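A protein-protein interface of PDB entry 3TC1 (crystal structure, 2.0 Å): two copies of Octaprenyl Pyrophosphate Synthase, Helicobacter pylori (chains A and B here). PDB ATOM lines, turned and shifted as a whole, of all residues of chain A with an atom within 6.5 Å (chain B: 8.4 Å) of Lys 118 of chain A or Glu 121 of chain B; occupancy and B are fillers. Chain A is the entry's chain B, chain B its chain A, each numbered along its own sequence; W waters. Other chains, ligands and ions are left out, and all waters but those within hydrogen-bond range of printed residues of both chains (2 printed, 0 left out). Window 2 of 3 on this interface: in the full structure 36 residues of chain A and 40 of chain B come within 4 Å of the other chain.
CE2 of Phe 113 of chain A touches CD2 of Leu 116 of chain B (3.7 Å). Phe 113 of chain A touches Ser 117 of chain B. Phe 113 of chain A touches Ser 128 of chain B (CD2 to CB, 3.5 Å). Phe 114 of chain A touches Gln 125 of chain B (CE1 to O, 3.5 Å). CA of Phe 114 of chain A touches OG of Ser 128 of chain B, at 3.2 Å. Ser 117 of chain A touches Glu 121 of chain B. CB of Ser 117 of chain A touches CB of Ala 124 of chain B (3.97 Å). Lys 118 of chain A touches Glu 121 of chain B. Lys 118 of chain A touches Gln 125 of chain B.
Of the 11 printed residues of chain A, 5 touch a printed residue of chain B. Printed residues of chain A that touch a printed residue of chain B: Phe 113, Phe 114, Ser 117, Lys 118 and Ala 124. Along chain A the printed residues that touch a printed residue of chain B span positions 113 to 124. Hydrophobic or aromatic side chains of chain B that line the printed part of chain A: Leu 116 and Ala 124. Among the printed residues, no Asp or Glu carboxylate lies within 4 Å of a Lys or Arg side-chain nitrogen of the other chain.
Water W1 lies within hydrogen-bond range of OE1 of Glu 121 of chain B (2.7 Å) and O of Lys 118 of chain A (3.5 Å). Water W2 lies within hydrogen-bond range of OE2 of Glu 121 of chain B (3.2 Å) and O of Lys 118 of chain A (3.5 Å).
The backbone carbonyl oxygen of Phe 114 of chain A is in hydrogen-bond range of the side-chain hydroxyl of Ser 117 of chain A. The side-chain hydroxyl (OG) of Ser 128 of chain B lies within hydrogen-bond range of the backbone carbonyl oxygen (O) of Ala 124 of chain B (2.9 Å). The side-chain amino group (NZ) of Lys 118 of chain A is in salt-bridge range of the side-chain carboxylate (OE1) of Glu 115 of chain A. The backbone carbonyl oxygen (O) of Gln 125 of chain B is in hydrogen-bond range of the side-chain hydroxyl (OG) of Ser 128 of chain B (3.4 Å). The side-chain carboxylate of Glu 121 of chain B lies within hydrogen-bond range of the side-chain amide nitrogen of Gln 125 of chain B (2.9 Å).
The side-chain amide nitrogen of Gln 125 of chain B sits close to the side-chain hydroxyl of Ser 117 of chain A, 3.5 Å away. The side-chain hydroxyl of Ser 117 of chain B is in hydrogen-bond range of the backbone carbonyl oxygen of Ala 124 of chain A, 3.4 Å away.
Ser 117 of chain A touches Ala 124 of chain B, and with the chains exchanged Ala 124 of chain A touches Ser 117 of chain B. Positions printed for both chains: 116, 117, 118, 119, 120 and 124.
Lys 118 of chain A touches two residues of chain B. Glu 121 of chain B touches just these residues of chain A: Ser 117 (3.8 Å) and Lys 118 (3.8 Å). Printed residues of chain A within 4 Å of Ser 117 of chain B: Phe 113 and Ala 124. Of the printed residues of chain B, Phe 114 of chain A touches Gln 125 and Ser 128. Met 119 of chain A touches none of the printed residues of chain B. The nearest residue of chain B that does not touch Lys 118 of chain A is Ala 124 of chain B (7.2 Å). The nearest printed residue of chain B that does not touch Phe 114 of chain A is Ala 126 of chain B (5.2 Å).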
ATOM      1  N   LYS A  58     -12.791 -16.671 -16.005  1.00  0.00           N
ATOM      2  CA  LYS A  58     -13.056 -17.736 -15.037  1.00  0.00           C
ATOM      3  C   LYS A  58     -14.263 -18.544 -15.500  1.00  0.00           C
ATOM      4  O   LYS A  58     -14.298 -19.762 -15.354  1.00  0.00           O
ATOM      5  CB  LYS A  58     -13.370 -17.163 -13.650  1.00  0.00           C
ATOM      6  CG  LYS A  58     -12.183 -16.690 -12.826  1.00  0.00           C
ATOM      7  CD  LYS A  58     -12.668 -16.346 -11.415  1.00  0.00           C
ATOM      8  CE  LYS A  58     -11.531 -16.050 -10.442  1.00  0.00           C
ATOM      9  NZ  LYS A  58     -11.016 -14.661 -10.549  1.00  0.00           N
ATOM     10  N   LYS A 111      -7.134 -33.595 -15.794  1.00  0.00           N
ATOM     11  CA  LYS A 111      -6.751 -32.242 -16.190  1.00  0.00           C
ATOM     12  C   LYS A 111      -7.889 -31.302 -15.811  1.00  0.00           C
ATOM     13  O   LYS A 111      -7.656 -30.198 -15.320  1.00  0.00           O
ATOM     14  CB  LYS A 111      -6.483 -32.166 -17.699  1.00  0.00           C
ATOM     15  CG  LYS A 111      -6.179 -30.751 -18.227  1.00  0.00           C
ATOM     16  CD  LYS A 111      -4.961 -30.108 -17.547  1.00  0.00           C
ATOM     17  CE  LYS A 111      -4.693 -28.710 -18.103  1.00  0.00           C
ATOM     18  NZ  LYS A 111      -3.579 -27.990 -17.419  1.00  0.00           N
ATOM     19  N   PHE A 113     -10.139 -31.710 -13.373  1.00  0.00           N
ATOM     20  CA  PHE A 113     -10.202 -31.543 -11.919  1.00  0.00           C
ATOM     21  C   PHE A 113      -9.068 -30.665 -11.420  1.00  0.00           C
ATOM     22  O   PHE A 113      -9.226 -29.923 -10.444  1.00  0.00           O
ATOM     23  CB  PHE A 113     -10.101 -32.884 -11.198  1.00  0.00           C
ATOM     24  CG  PHE A 113     -10.371 -32.796  -9.714  1.00  0.00           C
ATOM     25  CD1 PHE A 113     -11.677 -32.810  -9.226  1.00  0.00           C
ATOM     26  CD2 PHE A 113      -9.321 -32.683  -8.809  1.00  0.00           C
ATOM     27  CE1 PHE A 113     -11.930 -32.716  -7.853  1.00  0.00           C
ATOM     28  CE2 PHE A 113      -9.561 -32.587  -7.440  1.00  0.00           C
ATOM     29  CZ  PHE A 113     -10.871 -32.605  -6.960  1.00  0.00           C
ATOM     30  N   PHE A 114      -7.917 -30.768 -12.073  1.00  0.00           N
ATOM     31  CA  PHE A 114      -6.770 -29.969 -11.677  1.00  0.00           C
ATOM     32  C   PHE A 114      -7.144 -28.497 -11.780  1.00  0.00           C
ATOM     33  O   PHE A 114      -6.896 -27.717 -10.862  1.00  0.00           O
ATOM     34  CB  PHE A 114      -5.570 -30.266 -12.576  1.00  0.00           C
ATOM     35  CG  PHE A 114      -4.366 -29.415 -12.269  1.00  0.00           C
ATOM     36  CD1 PHE A 114      -3.568 -29.689 -11.165  1.00  0.00           C
ATOM     37  CD2 PHE A 114      -4.062 -28.307 -13.058  1.00  0.00           C
ATOM     38  CE1 PHE A 114      -2.484 -28.869 -10.847  1.00  0.00           C
ATOM     39  CE2 PHE A 114      -2.981 -27.480 -12.749  1.00  0.00           C
ATOM     40  CZ  PHE A 114      -2.191 -27.761 -11.642  1.00  0.00           C
ATOM     41  N   GLU A 115      -7.749 -28.124 -12.902  1.00  0.00           N
ATOM     42  CA  GLU A 115      -8.158 -26.747 -13.115  1.00  0.00           C
ATOM     43  C   GLU A 115      -9.329 -26.396 -12.194  1.00  0.00           C
ATOM     44  O   GLU A 115      -9.440 -25.264 -11.711  1.00  0.00           O
ATOM     45  CB  GLU A 115      -8.555 -26.542 -14.580  1.00  0.00           C
ATOM     46  CG  GLU A 115      -7.422 -26.756 -15.580  1.00  0.00           C
ATOM     47  CD  GLU A 115      -6.207 -25.884 -15.303  1.00  0.00           C
ATOM     48  OE1 GLU A 115      -6.375 -24.775 -14.759  1.00  0.00           O
ATOM     49  OE2 GLU A 115      -5.080 -26.303 -15.645  1.00  0.00           O
ATOM     50  N   LEU A 116     -10.190 -27.378 -11.943  1.00  0.00           N
ATOM     51  CA  LEU A 116     -11.364 -27.190 -11.089  1.00  0.00           C
ATOM     52  C   LEU A 116     -11.013 -26.726  -9.671  1.00  0.00           C
ATOM     53  O   LEU A 116     -11.740 -25.926  -9.068  1.00  0.00           O
ATOM     54  CB  LEU A 116     -12.170 -28.496 -11.019  1.00  0.00           C
ATOM     55  CG  LEU A 116     -13.448 -28.499 -10.172  1.00  0.00           C
ATOM     56  CD1 LEU A 116     -14.420 -27.431 -10.675  1.00  0.00           C
ATOM     57  CD2 LEU A 116     -14.099 -29.880 -10.242  1.00  0.00           C
ATOM     58  N   SER A 117      -9.899 -27.215  -9.147  1.00  0.00           N
ATOM     59  CA  SER A 117      -9.462 -26.850  -7.800  1.00  0.00           C
ATOM     60  C   SER A 117      -9.243 -25.344  -7.617  1.00  0.00           C
ATOM     61  O   SER A 117      -9.125 -24.858  -6.492  1.00  0.00           O
ATOM     62  CB  SER A 117      -8.173 -27.593  -7.461  1.00  0.00           C
ATOM     63  OG  SER A 117      -7.131 -27.197  -8.331  1.00  0.00           O
ATOM     64  N   LYS A 118      -9.192 -24.608  -8.720  1.00  0.00           N
ATOM     65  CA  LYS A 118      -8.977 -23.166  -8.659  1.00  0.00           C
ATOM     66  C   LYS A 118     -10.305 -22.420  -8.615  1.00  0.00           C
ATOM     67  O   LYS A 118     -10.340 -21.191  -8.508  1.00  0.00           O
ATOM     68  CB  LYS A 118      -8.174 -22.715  -9.882  1.00  0.00           C
ATOM     69  CG  LYS A 118      -6.863 -23.464 -10.076  1.00  0.00           C
ATOM     70  CD  LYS A 118      -6.227 -23.117 -11.413  1.00  0.00           C
ATOM     71  CE  LYS A 118      -4.936 -23.889 -11.630  1.00  0.00           C
ATOM     72  NZ  LYS A 118      -4.375 -23.672 -12.993  1.00  0.00           N
ATOM     73  N   MET A 119     -11.398 -23.171  -8.696  1.00  0.00           N
ATOM     74  CA  MET A 119     -12.739 -22.600  -8.688  1.00  0.00           C
ATOM     75  C   MET A 119     -13.316 -22.412  -7.287  1.00  0.00           C
ATOM     76  O   MET A 119     -14.325 -21.729  -7.114  1.00  0.00           O
ATOM     77  CB  MET A 119     -13.690 -23.493  -9.494  1.00  0.00           C
ATOM     78  CG  MET A 119     -13.447 -23.506 -10.999  1.00  0.00           C
ATOM     79  SD  MET A 119     -13.917 -21.947 -11.784  1.00  0.00           S
ATOM     80  CE  MET A 119     -12.861 -21.975 -13.219  1.00  0.00           C
ATOM     81  N   GLY A 120     -12.686 -23.012  -6.287  1.00  0.00           N
ATOM     82  CA  GLY A 120     -13.216 -22.890  -4.943  1.00  0.00           C
ATOM     83  C   GLY A 120     -13.948 -24.170  -4.575  1.00  0.00           C
ATOM     84  O   GLY A 120     -14.424 -24.897  -5.448  1.00  0.00           O
ATOM     85  N   ALA A 124     -16.084 -26.830  -6.852  1.00  0.00           N
ATOM     86  CA  ALA A 124     -15.322 -28.071  -6.976  1.00  0.00           C
ATOM     87  C   ALA A 124     -16.124 -29.270  -6.477  1.00  0.00           C
ATOM     88  O   ALA A 124     -16.082 -30.340  -7.077  1.00  0.00           O
ATOM     89  CB  ALA A 124     -14.007 -27.969  -6.206  1.00  0.00           C
ATOM     90  N   LEU B 116     -11.296 -35.078  -2.039  1.00  0.00           N
ATOM     91  CA  LEU B 116     -10.089 -34.270  -2.205  1.00  0.00           C
ATOM     92  C   LEU B 116     -10.505 -32.798  -2.334  1.00  0.00           C
ATOM     93  O   LEU B 116      -9.753 -31.894  -1.968  1.00  0.00           O
ATOM     94  CB  LEU B 116      -9.321 -34.721  -3.454  1.00  0.00           C
ATOM     95  CG  LEU B 116      -8.027 -33.996  -3.856  1.00  0.00           C
ATOM     96  CD1 LEU B 116      -6.985 -34.127  -2.751  1.00  0.00           C
ATOM     97  CD2 LEU B 116      -7.494 -34.586  -5.160  1.00  0.00           C
ATOM     98  N   SER B 117     -11.716 -32.582  -2.849  1.00  0.00           N
ATOM     99  CA  SER B 117     -12.283 -31.240  -3.036  1.00  0.00           C
ATOM    100  C   SER B 117     -12.285 -30.436  -1.752  1.00  0.00           C
ATOM    101  O   SER B 117     -12.277 -29.206  -1.766  1.00  0.00           O
ATOM    102  CB  SER B 117     -13.737 -31.327  -3.504  1.00  0.00           C
ATOM    103  OG  SER B 117     -13.849 -31.573  -4.890  1.00  0.00           O
ATOM    104  N   LYS B 118     -12.322 -31.153  -0.641  1.00  0.00           N
ATOM    105  CA  LYS B 118     -12.375 -30.541   0.674  1.00  0.00           C
ATOM    106  C   LYS B 118     -11.020 -30.320   1.315  1.00  0.00           C
ATOM    107  O   LYS B 118     -10.946 -29.833   2.441  1.00  0.00           O
ATOM    108  CB  LYS B 118     -13.199 -31.428   1.602  1.00  0.00           C
ATOM    109  CG  LYS B 118     -14.463 -31.965   0.979  1.00  0.00           C
ATOM    110  CD  LYS B 118     -15.174 -32.892   1.933  1.00  0.00           C
ATOM    111  CE  LYS B 118     -16.430 -33.452   1.310  1.00  0.00           C
ATOM    112  NZ  LYS B 118     -16.940 -34.589   2.119  1.00  0.00           N
ATOM    113  N   MET B 119      -9.945 -30.636   0.607  1.00  0.00           N
ATOM    114  CA  MET B 119      -8.624 -30.524   1.214  1.00  0.00           C
ATOM    115  C   MET B 119      -7.726 -29.309   1.048  1.00  0.00           C
ATOM    116  O   MET B 119      -6.651 -29.260   1.631  1.00  0.00           O
ATOM    117  CB  MET B 119      -7.820 -31.773   0.868  1.00  0.00           C
ATOM    118  CG  MET B 119      -8.472 -33.032   1.406  1.00  0.00           C
ATOM    119  SD  MET B 119      -7.361 -34.052   2.383  1.00  0.00           S
ATOM    120  CE  MET B 119      -6.455 -32.813   3.289  1.00  0.00           C
ATOM    121  N   GLY B 120      -8.139 -28.312   0.294  1.00  0.00           N
ATOM    122  CA  GLY B 120      -7.239 -27.187   0.146  1.00  0.00           C
ATOM    123  C   GLY B 120      -6.572 -27.331  -1.199  1.00  0.00           C
ATOM    124  O   GLY B 120      -6.196 -28.426  -1.627  1.00  0.00           O
ATOM    125  N   GLU B 121      -6.425 -26.196  -1.857  1.00  0.00           N
ATOM    126  CA  GLU B 121      -5.873 -26.117  -3.191  1.00  0.00           C
ATOM    127  C   GLU B 121      -4.542 -26.795  -3.483  1.00  0.00           C
ATOM    128  O   GLU B 121      -4.428 -27.510  -4.478  1.00  0.00           O
ATOM    129  CB  GLU B 121      -5.808 -24.651  -3.593  1.00  0.00           C
ATOM    130  CG  GLU B 121      -5.569 -24.428  -5.053  1.00  0.00           C
ATOM    131  CD  GLU B 121      -5.930 -23.023  -5.462  1.00  0.00           C
ATOM    132  OE1 GLU B 121      -5.629 -22.642  -6.611  1.00  0.00           O
ATOM    133  OE2 GLU B 121      -6.523 -22.301  -4.632  1.00  0.00           O
ATOM    134  N   LEU B 122      -3.538 -26.579  -2.640  1.00  0.00           N
ATOM    135  CA  LEU B 122      -2.228 -27.177  -2.871  1.00  0.00           C
ATOM    136  C   LEU B 122      -2.252 -28.701  -2.924  1.00  0.00           C
ATOM    137  O   LEU B 122      -1.637 -29.303  -3.802  1.00  0.00           O
ATOM    138  CB  LEU B 122      -1.228 -26.716  -1.805  1.00  0.00           C
ATOM    139  CG  LEU B 122      -0.774 -25.257  -1.872  1.00  0.00           C
ATOM    140  CD1 LEU B 122       0.183 -24.971  -0.720  1.00  0.00           C
ATOM    141  CD2 LEU B 122      -0.101 -24.984  -3.212  1.00  0.00           C
ATOM    142  N   ILE B 123      -2.953 -29.326  -1.983  1.00  0.00           N
ATOM    143  CA  ILE B 123      -3.033 -30.778  -1.962  1.00  0.00           C
ATOM    144  C   ILE B 123      -3.918 -31.274  -3.107  1.00  0.00           C
ATOM    145  O   ILE B 123      -3.606 -32.272  -3.761  1.00  0.00           O
ATOM    146  CB  ILE B 123      -3.567 -31.275  -0.591  1.00  0.00           C
ATOM    147  CG1 ILE B 123      -2.555 -30.919   0.505  1.00  0.00           C
ATOM    148  CG2 ILE B 123      -3.812 -32.780  -0.630  1.00  0.00           C
ATOM    149  CD1 ILE B 123      -3.006 -31.256   1.929  1.00  0.00           C
ATOM    150  N   ALA B 124      -5.016 -30.568  -3.363  1.00  0.00           N
ATOM    151  CA  ALA B 124      -5.912 -30.958  -4.441  1.00  0.00           C
ATOM    152  C   ALA B 124      -5.169 -30.941  -5.775  1.00  0.00           C
ATOM    153  O   ALA B 124      -5.348 -31.828  -6.610  1.00  0.00           O
ATOM    154  CB  ALA B 124      -7.113 -30.017  -4.496  1.00  0.00           C
ATOM    155  N   GLN B 125      -4.334 -29.929  -5.975  1.00  0.00           N
ATOM    156  CA  GLN B 125      -3.580 -29.818  -7.216  1.00  0.00           C
ATOM    157  C   GLN B 125      -2.451 -30.838  -7.315  1.00  0.00           C
ATOM    158  O   GLN B 125      -2.180 -31.364  -8.390  1.00  0.00           O
ATOM    159  CB  GLN B 125      -3.028 -28.400  -7.368  1.00  0.00           C
ATOM    160  CG  GLN B 125      -4.056 -27.431  -7.923  1.00  0.00           C
ATOM    161  CD  GLN B 125      -3.562 -26.003  -7.964  1.00  0.00           C
ATOM    162  OE1 GLN B 125      -2.379 -25.747  -8.186  1.00  0.00           O
ATOM    163  NE2 GLN B 125      -4.474 -25.059  -7.772  1.00  0.00           N
ATOM    164  N   ALA B 126      -1.802 -31.124  -6.194  1.00  0.00           N
ATOM    165  CA  ALA B 126      -0.707 -32.090  -6.182  1.00  0.00           C
ATOM    166  C   ALA B 126      -1.192 -33.473  -6.610  1.00  0.00           C
ATOM    167  O   ALA B 126      -0.595 -34.113  -7.478  1.00  0.00           O
ATOM    168  CB  ALA B 126      -0.092 -32.160  -4.787  1.00  0.00           C
ATOM    169  N   LEU B 127      -2.279 -33.932  -5.998  1.00  0.00           N
ATOM    170  CA  LEU B 127      -2.818 -35.244  -6.316  1.00  0.00           C
ATOM    171  C   LEU B 127      -3.511 -35.322  -7.673  1.00  0.00           C
ATOM    172  O   LEU B 127      -3.376 -36.325  -8.377  1.00  0.00           O
ATOM    173  CB  LEU B 127      -3.760 -35.706  -5.201  1.00  0.00           C
ATOM    174  CG  LEU B 127      -3.071 -35.901  -3.842  1.00  0.00           C
ATOM    175  CD1 LEU B 127      -4.063 -36.457  -2.823  1.00  0.00           C
ATOM    176  CD2 LEU B 127      -1.881 -36.853  -4.003  1.00  0.00           C
ATOM    177  N   SER B 128      -4.246 -34.283  -8.063  1.00  0.00           N
ATOM    178  CA  SER B 128      -4.909 -34.346  -9.361  1.00  0.00           C
ATOM    179  C   SER B 128      -3.856 -34.308 -10.470  1.00  0.00           C
ATOM    180  O   SER B 128      -3.996 -34.974 -11.495  1.00  0.00           O
ATOM    181  CB  SER B 128      -5.929 -33.205  -9.529  1.00  0.00           C
ATOM    182  OG  SER B 128      -5.322 -31.928  -9.556  1.00  0.00           O
ATOM    183  N   SER B 173       2.049 -34.114  -0.324  1.00  0.00           N
ATOM    184  CA  SER B 173       0.731 -33.748   0.181  1.00  0.00           C
ATOM    185  C   SER B 173       0.591 -33.936   1.691  1.00  0.00           C
ATOM    186  O   SER B 173      -0.012 -33.100   2.365  1.00  0.00           O
ATOM    187  CB  SER B 173      -0.357 -34.555  -0.530  1.00  0.00           C
ATOM    188  OG  SER B 173      -0.437 -34.196  -1.898  1.00  0.00           O
ATOM    189  N   ILE B 176       2.556 -31.205   3.444  1.00  0.00           N
ATOM    190  CA  ILE B 176       1.799 -29.955   3.451  1.00  0.00           C
ATOM    191  C   ILE B 176       0.756 -29.990   4.572  1.00  0.00           C
ATOM    192  O   ILE B 176       0.670 -29.071   5.390  1.00  0.00           O
ATOM    193  CB  ILE B 176       1.069 -29.739   2.096  1.00  0.00           C
ATOM    194  CG1 ILE B 176       2.099 -29.469   0.993  1.00  0.00           C
ATOM    195  CG2 ILE B 176       0.058 -28.587   2.215  1.00  0.00           C
ATOM    196  CD1 ILE B 176       1.499 -29.330  -0.398  1.00  0.00           C
HETATM  197  O   HOH W   1      -7.083 -20.555  -7.467  1.00  0.00           O
HETATM  198  O   HOH W   2      -9.649 -21.584  -5.125  1.00  0.00           O
